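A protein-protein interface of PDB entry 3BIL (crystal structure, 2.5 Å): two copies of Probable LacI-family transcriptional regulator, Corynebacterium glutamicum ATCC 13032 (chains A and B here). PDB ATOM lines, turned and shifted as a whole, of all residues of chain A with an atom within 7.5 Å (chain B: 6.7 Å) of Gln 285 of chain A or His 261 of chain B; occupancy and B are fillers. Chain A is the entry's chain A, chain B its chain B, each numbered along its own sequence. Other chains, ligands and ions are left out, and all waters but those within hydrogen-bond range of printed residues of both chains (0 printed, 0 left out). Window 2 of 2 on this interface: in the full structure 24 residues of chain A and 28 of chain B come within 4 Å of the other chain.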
ATOM      1  N   ILE A 257      -6.161   2.047   6.385  1.00  0.00           N
ATOM      2  CA  ILE A 257      -6.562   0.622   6.391  1.00  0.00           C
ATOM      3  C   ILE A 257      -8.049   0.495   6.045  1.00  0.00           C
ATOM      4  O   ILE A 257      -8.445  -0.254   5.125  1.00  0.00           O
ATOM      5  CB  ILE A 257      -6.226  -0.104   7.727  1.00  0.00           C
ATOM      6  CG1 ILE A 257      -4.705  -0.196   7.917  1.00  0.00           C
ATOM      7  CG2 ILE A 257      -6.765  -1.501   7.709  1.00  0.00           C
ATOM      8  CD1 ILE A 257      -4.215  -0.433   9.379  1.00  0.00           C
ATOM      9  N   ILE A 267      -3.358  -4.371   0.588  1.00  0.00           N
ATOM     10  CA  ILE A 267      -2.117  -3.731   0.943  1.00  0.00           C
ATOM     11  C   ILE A 267      -0.926  -4.636   0.704  1.00  0.00           C
ATOM     12  O   ILE A 267      -1.006  -5.855   0.916  1.00  0.00           O
ATOM     13  CB  ILE A 267      -2.110  -3.296   2.403  1.00  0.00           C
ATOM     14  CG1 ILE A 267      -3.266  -2.323   2.603  1.00  0.00           C
ATOM     15  CG2 ILE A 267      -0.699  -2.694   2.773  1.00  0.00           C
ATOM     16  CD1 ILE A 267      -3.293  -1.597   3.877  1.00  0.00           C
ATOM     17  N   PRO A 280       0.666  -2.967  17.863  1.00  0.00           N
ATOM     18  CA  PRO A 280       0.850  -4.428  17.699  1.00  0.00           C
ATOM     19  C   PRO A 280       0.103  -5.029  16.505  1.00  0.00           C
ATOM     20  O   PRO A 280       0.668  -5.865  15.772  1.00  0.00           O
ATOM     21  CB  PRO A 280       0.356  -5.023  19.033  1.00  0.00           C
ATOM     22  CG  PRO A 280      -0.111  -3.817  19.885  1.00  0.00           C
ATOM     23  CD  PRO A 280       0.426  -2.574  19.271  1.00  0.00           C
ATOM     24  N   LEU A 281      -1.129  -4.581  16.280  1.00  0.00           N
ATOM     25  CA  LEU A 281      -1.906  -5.089  15.135  1.00  0.00           C
ATOM     26  C   LEU A 281      -1.429  -4.661  13.748  1.00  0.00           C
ATOM     27  O   LEU A 281      -1.788  -5.321  12.767  1.00  0.00           O
ATOM     28  CB  LEU A 281      -3.419  -4.858  15.293  1.00  0.00           C
ATOM     29  CG  LEU A 281      -4.126  -5.701  16.366  1.00  0.00           C
ATOM     30  CD1 LEU A 281      -5.622  -5.341  16.508  1.00  0.00           C
ATOM     31  CD2 LEU A 281      -3.943  -7.207  16.106  1.00  0.00           C
ATOM     32  N   PHE A 282      -0.619  -3.591  13.648  1.00  0.00           N
ATOM     33  CA  PHE A 282       0.010  -3.254  12.349  1.00  0.00           C
ATOM     34  C   PHE A 282       0.981  -4.351  11.909  1.00  0.00           C
ATOM     35  O   PHE A 282       1.025  -4.691  10.744  1.00  0.00           O
ATOM     36  CB  PHE A 282       0.654  -1.839  12.284  1.00  0.00           C
ATOM     37  CG  PHE A 282      -0.324  -0.671  12.507  1.00  0.00           C
ATOM     38  CD1 PHE A 282       0.169   0.585  12.860  1.00  0.00           C
ATOM     39  CD2 PHE A 282      -1.705  -0.833  12.358  1.00  0.00           C
ATOM     40  CE1 PHE A 282      -0.667   1.650  13.102  1.00  0.00           C
ATOM     41  CE2 PHE A 282      -2.573   0.228  12.560  1.00  0.00           C
ATOM     42  CZ  PHE A 282      -2.064   1.481  12.951  1.00  0.00           C
ATOM     43  N   ALA A 283       1.695  -4.963  12.846  1.00  0.00           N
ATOM     44  CA  ALA A 283       2.698  -5.989  12.508  1.00  0.00           C
ATOM     45  C   ALA A 283       2.104  -7.333  12.081  1.00  0.00           C
ATOM     46  O   ALA A 283       2.846  -8.235  11.651  1.00  0.00           O
ATOM     47  CB  ALA A 283       3.622  -6.190  13.688  1.00  0.00           C
ATOM     48  N   LEU A 284       0.779  -7.475  12.214  1.00  0.00           N
ATOM     49  CA  LEU A 284       0.112  -8.777  12.040  1.00  0.00           C
ATOM     50  C   LEU A 284      -0.982  -8.826  10.955  1.00  0.00           C
ATOM     51  O   LEU A 284      -1.726  -9.810  10.885  1.00  0.00           O
ATOM     52  CB  LEU A 284      -0.475  -9.291  13.379  1.00  0.00           C
ATOM     53  CG  LEU A 284       0.338  -9.187  14.673  1.00  0.00           C
ATOM     54  CD1 LEU A 284      -0.576  -9.423  15.834  1.00  0.00           C
ATOM     55  CD2 LEU A 284       1.563 -10.101  14.720  1.00  0.00           C
ATOM     56  N   GLN A 285      -1.094  -7.758  10.157  1.00  0.00           N
ATOM     57  CA  GLN A 285      -1.833  -7.745   8.893  1.00  0.00           C
ATOM     58  C   GLN A 285      -1.296  -8.886   7.974  1.00  0.00           C
ATOM     59  O   GLN A 285      -0.173  -9.357   8.187  1.00  0.00           O
ATOM     60  CB  GLN A 285      -1.676  -6.360   8.198  1.00  0.00           C
ATOM     61  CG  GLN A 285      -2.150  -5.071   8.963  1.00  0.00           C
ATOM     62  CD  GLN A 285      -3.631  -5.090   9.418  1.00  0.00           C
ATOM     63  OE1 GLN A 285      -4.569  -4.914   8.605  1.00  0.00           O
ATOM     64  NE2 GLN A 285      -3.840  -5.291  10.733  1.00  0.00           N
ATOM     65  N   PRO A 286      -2.088  -9.364   6.979  1.00  0.00           N
ATOM     66  CA  PRO A 286      -1.539 -10.363   6.014  1.00  0.00           C
ATOM     67  C   PRO A 286      -0.240  -9.927   5.346  1.00  0.00           C
ATOM     68  O   PRO A 286       0.590 -10.767   5.016  1.00  0.00           O
ATOM     69  CB  PRO A 286      -2.652 -10.528   4.958  1.00  0.00           C
ATOM     70  CG  PRO A 286      -3.610  -9.361   5.214  1.00  0.00           C
ATOM     71  CD  PRO A 286      -3.506  -9.073   6.705  1.00  0.00           C
ATOM     72  N   HIS A 287      -0.069  -8.635   5.110  1.00  0.00           N
ATOM     73  CA  HIS A 287       1.237  -8.124   4.749  1.00  0.00           C
ATOM     74  C   HIS A 287       1.573  -7.066   5.790  1.00  0.00           C
ATOM     75  O   HIS A 287       0.989  -5.976   5.810  1.00  0.00           O
ATOM     76  CB  HIS A 287       1.253  -7.536   3.356  1.00  0.00           C
ATOM     77  CG  HIS A 287       1.025  -8.535   2.266  1.00  0.00           C
ATOM     78  ND1 HIS A 287      -0.212  -9.106   2.023  1.00  0.00           N
ATOM     79  CD2 HIS A 287       1.869  -9.046   1.337  1.00  0.00           C
ATOM     80  CE1 HIS A 287      -0.113  -9.936   0.997  1.00  0.00           C
ATOM     81  NE2 HIS A 287       1.136  -9.917   0.564  1.00  0.00           N
ATOM     82  N   PRO A 288       2.486  -7.396   6.699  1.00  0.00           N
ATOM     83  CA  PRO A 288       2.702  -6.444   7.767  1.00  0.00           C
ATOM     84  C   PRO A 288       3.048  -5.058   7.221  1.00  0.00           C
ATOM     85  O   PRO A 288       3.520  -4.944   6.089  1.00  0.00           O
ATOM     86  CB  PRO A 288       3.855  -7.076   8.546  1.00  0.00           C
ATOM     87  CG  PRO A 288       3.666  -8.570   8.278  1.00  0.00           C
ATOM     88  CD  PRO A 288       3.343  -8.586   6.835  1.00  0.00           C
ATOM     89  N   LEU A 289       2.795  -4.024   8.022  1.00  0.00           N
ATOM     90  CA  LEU A 289       2.902  -2.674   7.555  1.00  0.00           C
ATOM     91  C   LEU A 289       4.262  -2.073   7.816  1.00  0.00           C
ATOM     92  O   LEU A 289       4.691  -1.996   8.948  1.00  0.00           O
ATOM     93  CB  LEU A 289       1.865  -1.792   8.235  1.00  0.00           C
ATOM     94  CG  LEU A 289       0.699  -1.216   7.479  1.00  0.00           C
ATOM     95  CD1 LEU A 289      -0.217  -2.327   6.968  1.00  0.00           C
ATOM     96  CD2 LEU A 289      -0.006  -0.348   8.474  1.00  0.00           C
ATOM     97  N   GLU A 331       6.280  -5.420   5.060  1.00  0.00           N
ATOM     98  CA  GLU A 331       5.925  -5.866   3.700  1.00  0.00           C
ATOM     99  C   GLU A 331       4.788  -5.145   2.928  1.00  0.00           C
ATOM    100  O   GLU A 331       4.131  -5.759   2.085  1.00  0.00           O
ATOM    101  CB  GLU A 331       5.699  -7.374   3.690  1.00  0.00           C
ATOM    102  CG  GLU A 331       6.957  -8.184   3.343  1.00  0.00           C
ATOM    103  CD  GLU A 331       7.641  -8.830   4.560  1.00  0.00           C
ATOM    104  OE1 GLU A 331       8.906  -8.851   4.587  1.00  0.00           O
ATOM    105  OE2 GLU A 331       6.913  -9.322   5.470  1.00  0.00           O
ATOM    106  N   SER A 332       4.576  -3.850   3.176  1.00  0.00           N
ATOM    107  CA  SER A 332       3.449  -3.135   2.560  1.00  0.00           C
ATOM    108  C   SER A 332       3.799  -2.202   1.363  1.00  0.00           C
ATOM    109  O   SER A 332       3.007  -1.325   1.005  1.00  0.00           O
ATOM    110  CB  SER A 332       2.683  -2.378   3.637  1.00  0.00           C
ATOM    111  OG  SER A 332       3.524  -1.585   4.452  1.00  0.00           O
ATOM    112  N   VAL B 256      -4.266 -14.443  19.807  1.00  0.00           N
ATOM    113  CA  VAL B 256      -4.906 -15.301  18.781  1.00  0.00           C
ATOM    114  C   VAL B 256      -4.579 -14.918  17.341  1.00  0.00           C
ATOM    115  O   VAL B 256      -4.316 -15.815  16.515  1.00  0.00           O
ATOM    116  CB  VAL B 256      -6.480 -15.438  18.956  1.00  0.00           C
ATOM    117  CG1 VAL B 256      -7.105 -16.067  17.715  1.00  0.00           C
ATOM    118  CG2 VAL B 256      -6.786 -16.259  20.168  1.00  0.00           C
ATOM    119  N   ILE B 257      -4.590 -13.603  17.042  1.00  0.00           N
ATOM    120  CA  ILE B 257      -4.232 -13.125  15.687  1.00  0.00           C
ATOM    121  C   ILE B 257      -2.781 -13.418  15.371  1.00  0.00           C
ATOM    122  O   ILE B 257      -2.463 -13.947  14.275  1.00  0.00           O
ATOM    123  CB  ILE B 257      -4.584 -11.609  15.431  1.00  0.00           C
ATOM    124  CG1 ILE B 257      -6.110 -11.402  15.424  1.00  0.00           C
ATOM    125  CG2 ILE B 257      -4.033 -11.167  14.100  1.00  0.00           C
ATOM    126  CD1 ILE B 257      -6.571  -9.936  15.644  1.00  0.00           C
ATOM    127  N   GLU B 258      -1.906 -13.104  16.327  1.00  0.00           N
ATOM    128  CA  GLU B 258      -0.458 -13.379  16.205  1.00  0.00           C
ATOM    129  C   GLU B 258      -0.210 -14.872  15.959  1.00  0.00           C
ATOM    130  O   GLU B 258       0.586 -15.262  15.062  1.00  0.00           O
ATOM    131  CB  GLU B 258       0.252 -12.909  17.461  1.00  0.00           C
ATOM    132  CG  GLU B 258       1.812 -13.056  17.528  1.00  0.00           C
ATOM    133  CD  GLU B 258       2.395 -12.519  18.888  1.00  0.00           C
ATOM    134  OE1 GLU B 258       3.588 -12.771  19.165  1.00  0.00           O
ATOM    135  OE2 GLU B 258       1.647 -11.877  19.704  1.00  0.00           O
ATOM    136  N   ALA B 259      -0.928 -15.704  16.723  1.00  0.00           N
ATOM    137  CA  ALA B 259      -0.825 -17.152  16.576  1.00  0.00           C
ATOM    138  C   ALA B 259      -1.194 -17.632  15.185  1.00  0.00           C
ATOM    139  O   ALA B 259      -0.492 -18.477  14.669  1.00  0.00           O
ATOM    140  CB  ALA B 259      -1.649 -17.860  17.623  1.00  0.00           C
ATOM    141  N   CYS B 260      -2.263 -17.087  14.571  1.00  0.00           N
ATOM    142  CA  CYS B 260      -2.660 -17.478  13.196  1.00  0.00           C
ATOM    143  C   CYS B 260      -1.731 -16.952  12.140  1.00  0.00           C
ATOM    144  O   CYS B 260      -1.511 -17.635  11.100  1.00  0.00           O
ATOM    145  CB  CYS B 260      -4.087 -17.039  12.853  1.00  0.00           C
ATOM    146  SG  CYS B 260      -5.242 -17.651  14.083  1.00  0.00           S
ATOM    147  N   HIS B 261      -1.209 -15.745  12.384  1.00  0.00           N
ATOM    148  CA  HIS B 261      -0.214 -15.146  11.484  1.00  0.00           C
ATOM    149  C   HIS B 261       1.093 -15.919  11.523  1.00  0.00           C
ATOM    150  O   HIS B 261       1.549 -16.385  10.476  1.00  0.00           O
ATOM    151  CB  HIS B 261       0.027 -13.651  11.779  1.00  0.00           C
ATOM    152  CG  HIS B 261       1.089 -13.015  10.925  1.00  0.00           C
ATOM    153  ND1 HIS B 261       0.899 -12.708   9.592  1.00  0.00           N
ATOM    154  CD2 HIS B 261       2.343 -12.600  11.227  1.00  0.00           C
ATOM    155  CE1 HIS B 261       1.990 -12.145   9.105  1.00  0.00           C
ATOM    156  NE2 HIS B 261       2.882 -12.069  10.075  1.00  0.00           N
ATOM    157  N   LYS B 262       1.692 -16.064  12.711  1.00  0.00           N
ATOM    158  CA  LYS B 262       2.954 -16.821  12.838  1.00  0.00           C
ATOM    159  C   LYS B 262       2.800 -18.190  12.187  1.00  0.00           C
ATOM    160  O   LYS B 262       3.680 -18.643  11.477  1.00  0.00           O
ATOM    161  CB  LYS B 262       3.404 -16.968  14.306  1.00  0.00           C
ATOM    162  CG  LYS B 262       4.008 -15.683  14.934  1.00  0.00           C
ATOM    163  CD  LYS B 262       5.568 -15.710  15.012  1.00  0.00           C
ATOM    164  CE  LYS B 262       6.156 -14.355  15.450  1.00  0.00           C
ATOM    165  NZ  LYS B 262       5.445 -13.631  16.566  1.00  0.00           N
ATOM    166  N   ALA B 263       1.652 -18.819  12.420  1.00  0.00           N
ATOM    167  CA  ALA B 263       1.334 -20.146  11.911  1.00  0.00           C
ATOM    168  C   ALA B 263       1.012 -20.192  10.409  1.00  0.00           C
ATOM    169  O   ALA B 263       0.968 -21.264   9.825  1.00  0.00           O
ATOM    170  CB  ALA B 263       0.165 -20.734  12.721  1.00  0.00           C
ATOM    171  N   GLY B 264       0.744 -19.046   9.795  1.00  0.00           N
ATOM    172  CA  GLY B 264       0.333 -19.015   8.385  1.00  0.00           C
ATOM    173  C   GLY B 264      -1.128 -19.385   8.152  1.00  0.00           C
ATOM    174  O   GLY B 264      -1.495 -19.857   7.084  1.00  0.00           O
ATOM    175  N   LEU B 265      -1.991 -19.159   9.131  1.00  0.00           N
ATOM    176  CA  LEU B 265      -3.384 -19.532   8.902  1.00  0.00           C
ATOM    177  C   LEU B 265      -4.244 -18.313   8.497  1.00  0.00           C
ATOM    178  O   LEU B 265      -4.169 -17.267   9.140  1.00  0.00           O
ATOM    179  CB  LEU B 265      -3.941 -20.268  10.136  1.00  0.00           C
ATOM    180  CG  LEU B 265      -3.126 -21.510  10.576  1.00  0.00           C
ATOM    181  CD1 LEU B 265      -3.416 -21.859  12.024  1.00  0.00           C
ATOM    182  CD2 LEU B 265      -3.379 -22.750   9.707  1.00  0.00           C
ATOM    183  N   ILE B 267      -7.462 -16.666   8.921  1.00  0.00           N
ATOM    184  CA  ILE B 267      -8.702 -16.564   9.653  1.00  0.00           C
ATOM    185  C   ILE B 267      -9.856 -16.384   8.687  1.00  0.00           C
ATOM    186  O   ILE B 267      -9.746 -15.612   7.711  1.00  0.00           O
ATOM    187  CB  ILE B 267      -8.718 -15.342  10.539  1.00  0.00           C
ATOM    188  CG1 ILE B 267      -7.520 -15.412  11.486  1.00  0.00           C
ATOM    189  CG2 ILE B 267     -10.060 -15.257  11.206  1.00  0.00           C
ATOM    190  CD1 ILE B 267      -7.486 -14.458  12.560  1.00  0.00           C
ATOM    191  N   LEU B 281      -9.707  -1.961  14.513  1.00  0.00           N
ATOM    192  CA  LEU B 281      -8.886  -2.766  13.614  1.00  0.00           C
ATOM    193  C   LEU B 281      -9.348  -4.213  13.396  1.00  0.00           C
ATOM    194  O   LEU B 281      -9.070  -4.818  12.336  1.00  0.00           O
ATOM    195  CB  LEU B 281      -7.420  -2.681  14.043  1.00  0.00           C
ATOM    196  CG  LEU B 281      -6.722  -1.475  13.386  1.00  0.00           C
ATOM    197  CD1 LEU B 281      -5.294  -1.318  13.888  1.00  0.00           C
ATOM    198  CD2 LEU B 281      -6.741  -1.708  11.861  1.00  0.00           C
ATOM    199  N   LEU B 284     -11.645  -4.696  10.419  1.00  0.00           N
ATOM    200  CA  LEU B 284     -10.998  -4.387   9.127  1.00  0.00           C
ATOM    201  C   LEU B 284     -10.167  -5.493   8.453  1.00  0.00           C
ATOM    202  O   LEU B 284     -10.126  -5.547   7.221  1.00  0.00           O
ATOM    203  CB  LEU B 284     -10.233  -3.037   9.169  1.00  0.00           C
ATOM    204  CG  LEU B 284     -11.104  -1.795   9.468  1.00  0.00           C
ATOM    205  CD1 LEU B 284     -10.284  -0.593   9.909  1.00  0.00           C
ATOM    206  CD2 LEU B 284     -12.081  -1.445   8.322  1.00  0.00           C
ATOM    207  N   GLN B 285      -9.510  -6.341   9.251  1.00  0.00           N
ATOM    208  CA  GLN B 285      -8.900  -7.595   8.792  1.00  0.00           C
ATOM    209  C   GLN B 285      -9.484  -8.090   7.447  1.00  0.00           C
ATOM    210  O   GLN B 285     -10.669  -7.860   7.172  1.00  0.00           O
ATOM    211  CB  GLN B 285      -9.069  -8.709   9.864  1.00  0.00           C
ATOM    212  CG  GLN B 285      -8.542  -8.435  11.316  1.00  0.00           C
ATOM    213  CD  GLN B 285      -6.995  -8.256  11.452  1.00  0.00           C
ATOM    214  OE1 GLN B 285      -6.176  -9.059  10.930  1.00  0.00           O
ATOM    215  NE2 GLN B 285      -6.605  -7.202  12.176  1.00  0.00           N
ATOM    216  N   PRO B 286      -8.671  -8.789   6.605  1.00  0.00           N
ATOM    217  CA  PRO B 286      -9.173  -9.341   5.309  1.00  0.00           C
ATOM    218  C   PRO B 286     -10.490 -10.109   5.443  1.00  0.00           C
ATOM    219  O   PRO B 286     -11.362  -9.990   4.573  1.00  0.00           O
ATOM    220  CB  PRO B 286      -8.051 -10.285   4.851  1.00  0.00           C
ATOM    221  CG  PRO B 286      -7.106 -10.415   6.095  1.00  0.00           C
ATOM    222  CD  PRO B 286      -7.242  -9.102   6.814  1.00  0.00           C
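Hydrophobic or aromatic side chains of chain B that line the printed part of chain A: Ile 257, His 261, Leu 281 and Pro 286.
Of the 14 printed residues of chain A, 6 touch a printed residue of chain B.
Hydrophobic or aromatic side chains of chain A within 4 Å of the printed part of chain B: Ile 257, Leu 281, Phe 282, Leu 284 and Pro 286.
Among the printed residues, 7 pairs touch across the chains.
Among the printed residues, no Asp or Glu carboxylate lies within 4 Å of a Lys or Arg side-chain nitrogen of the other chain.
Ile 257 of chain A touches Leu 281 of chain B, and with the chains exchanged Leu 281 of chain A touches Ile 257 of chain B.
Gln 285 of chain B touches its own counterpart, Gln 285 of chain A.
Pro 286 of chain B touches its own counterpart, Pro 286 of chain A.
6 positions are printed for both chains.
The backbone carbonyl oxygen (O) of Leu 281 of chain A lies within hydrogen-bond range of the side-chain amide nitrogen (NE2) of Gln 285 of chain A.
N of Leu 289 of chain A lies within hydrogen-bond range of O of Phe 282 of chain A, at 3.3 Å.
The side-chain carboxylate of Glu 258 of chain B is in salt-bridge range of the side-chain amino group of Lys 262 of chain B (3.3 Å).
The side-chain amide nitrogen (NE2) of Gln 285 of chain B is in hydrogen-bond range of the backbone carbonyl oxygen (O) of Leu 281 of chain B (3.4 Å).
Gln 285 of chain A touches just these residues of chain B: His 261 and Gln 285.
Of the printed residues of chain A, His 261 of chain B touches Gln 285 (3.6 Å).
Of the printed residues of chain B, Ile 257 of chain A touches Leu 281 (3.8 Å).
Printed residues of chain A within 4 Å of Ile 257 of chain B: Leu 281.
The nearest printed residue of chain A that does not touch His 261 of chain B is Pro 288 of chain A (4.01 Å).
The nearest printed residue of chain A that does not touch Ile 257 of chain B is Leu 284 of chain A (4.1 Å).
Among the printed residues, merely in contact across the chains: Ile 257 of chain A with Leu 281 of chain B, Leu 281 of chain A with Ile 257 of chain B, Phe 282 of chain A with Leu 281 of chain B, Leu 284 of chain A with Glu 258 of chain B, Gln 285 of chain A with His 261 of chain B, Gln 285 of chain A with Gln 285 of chain B and Pro 286 of chain A with Pro 286 of chain B.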
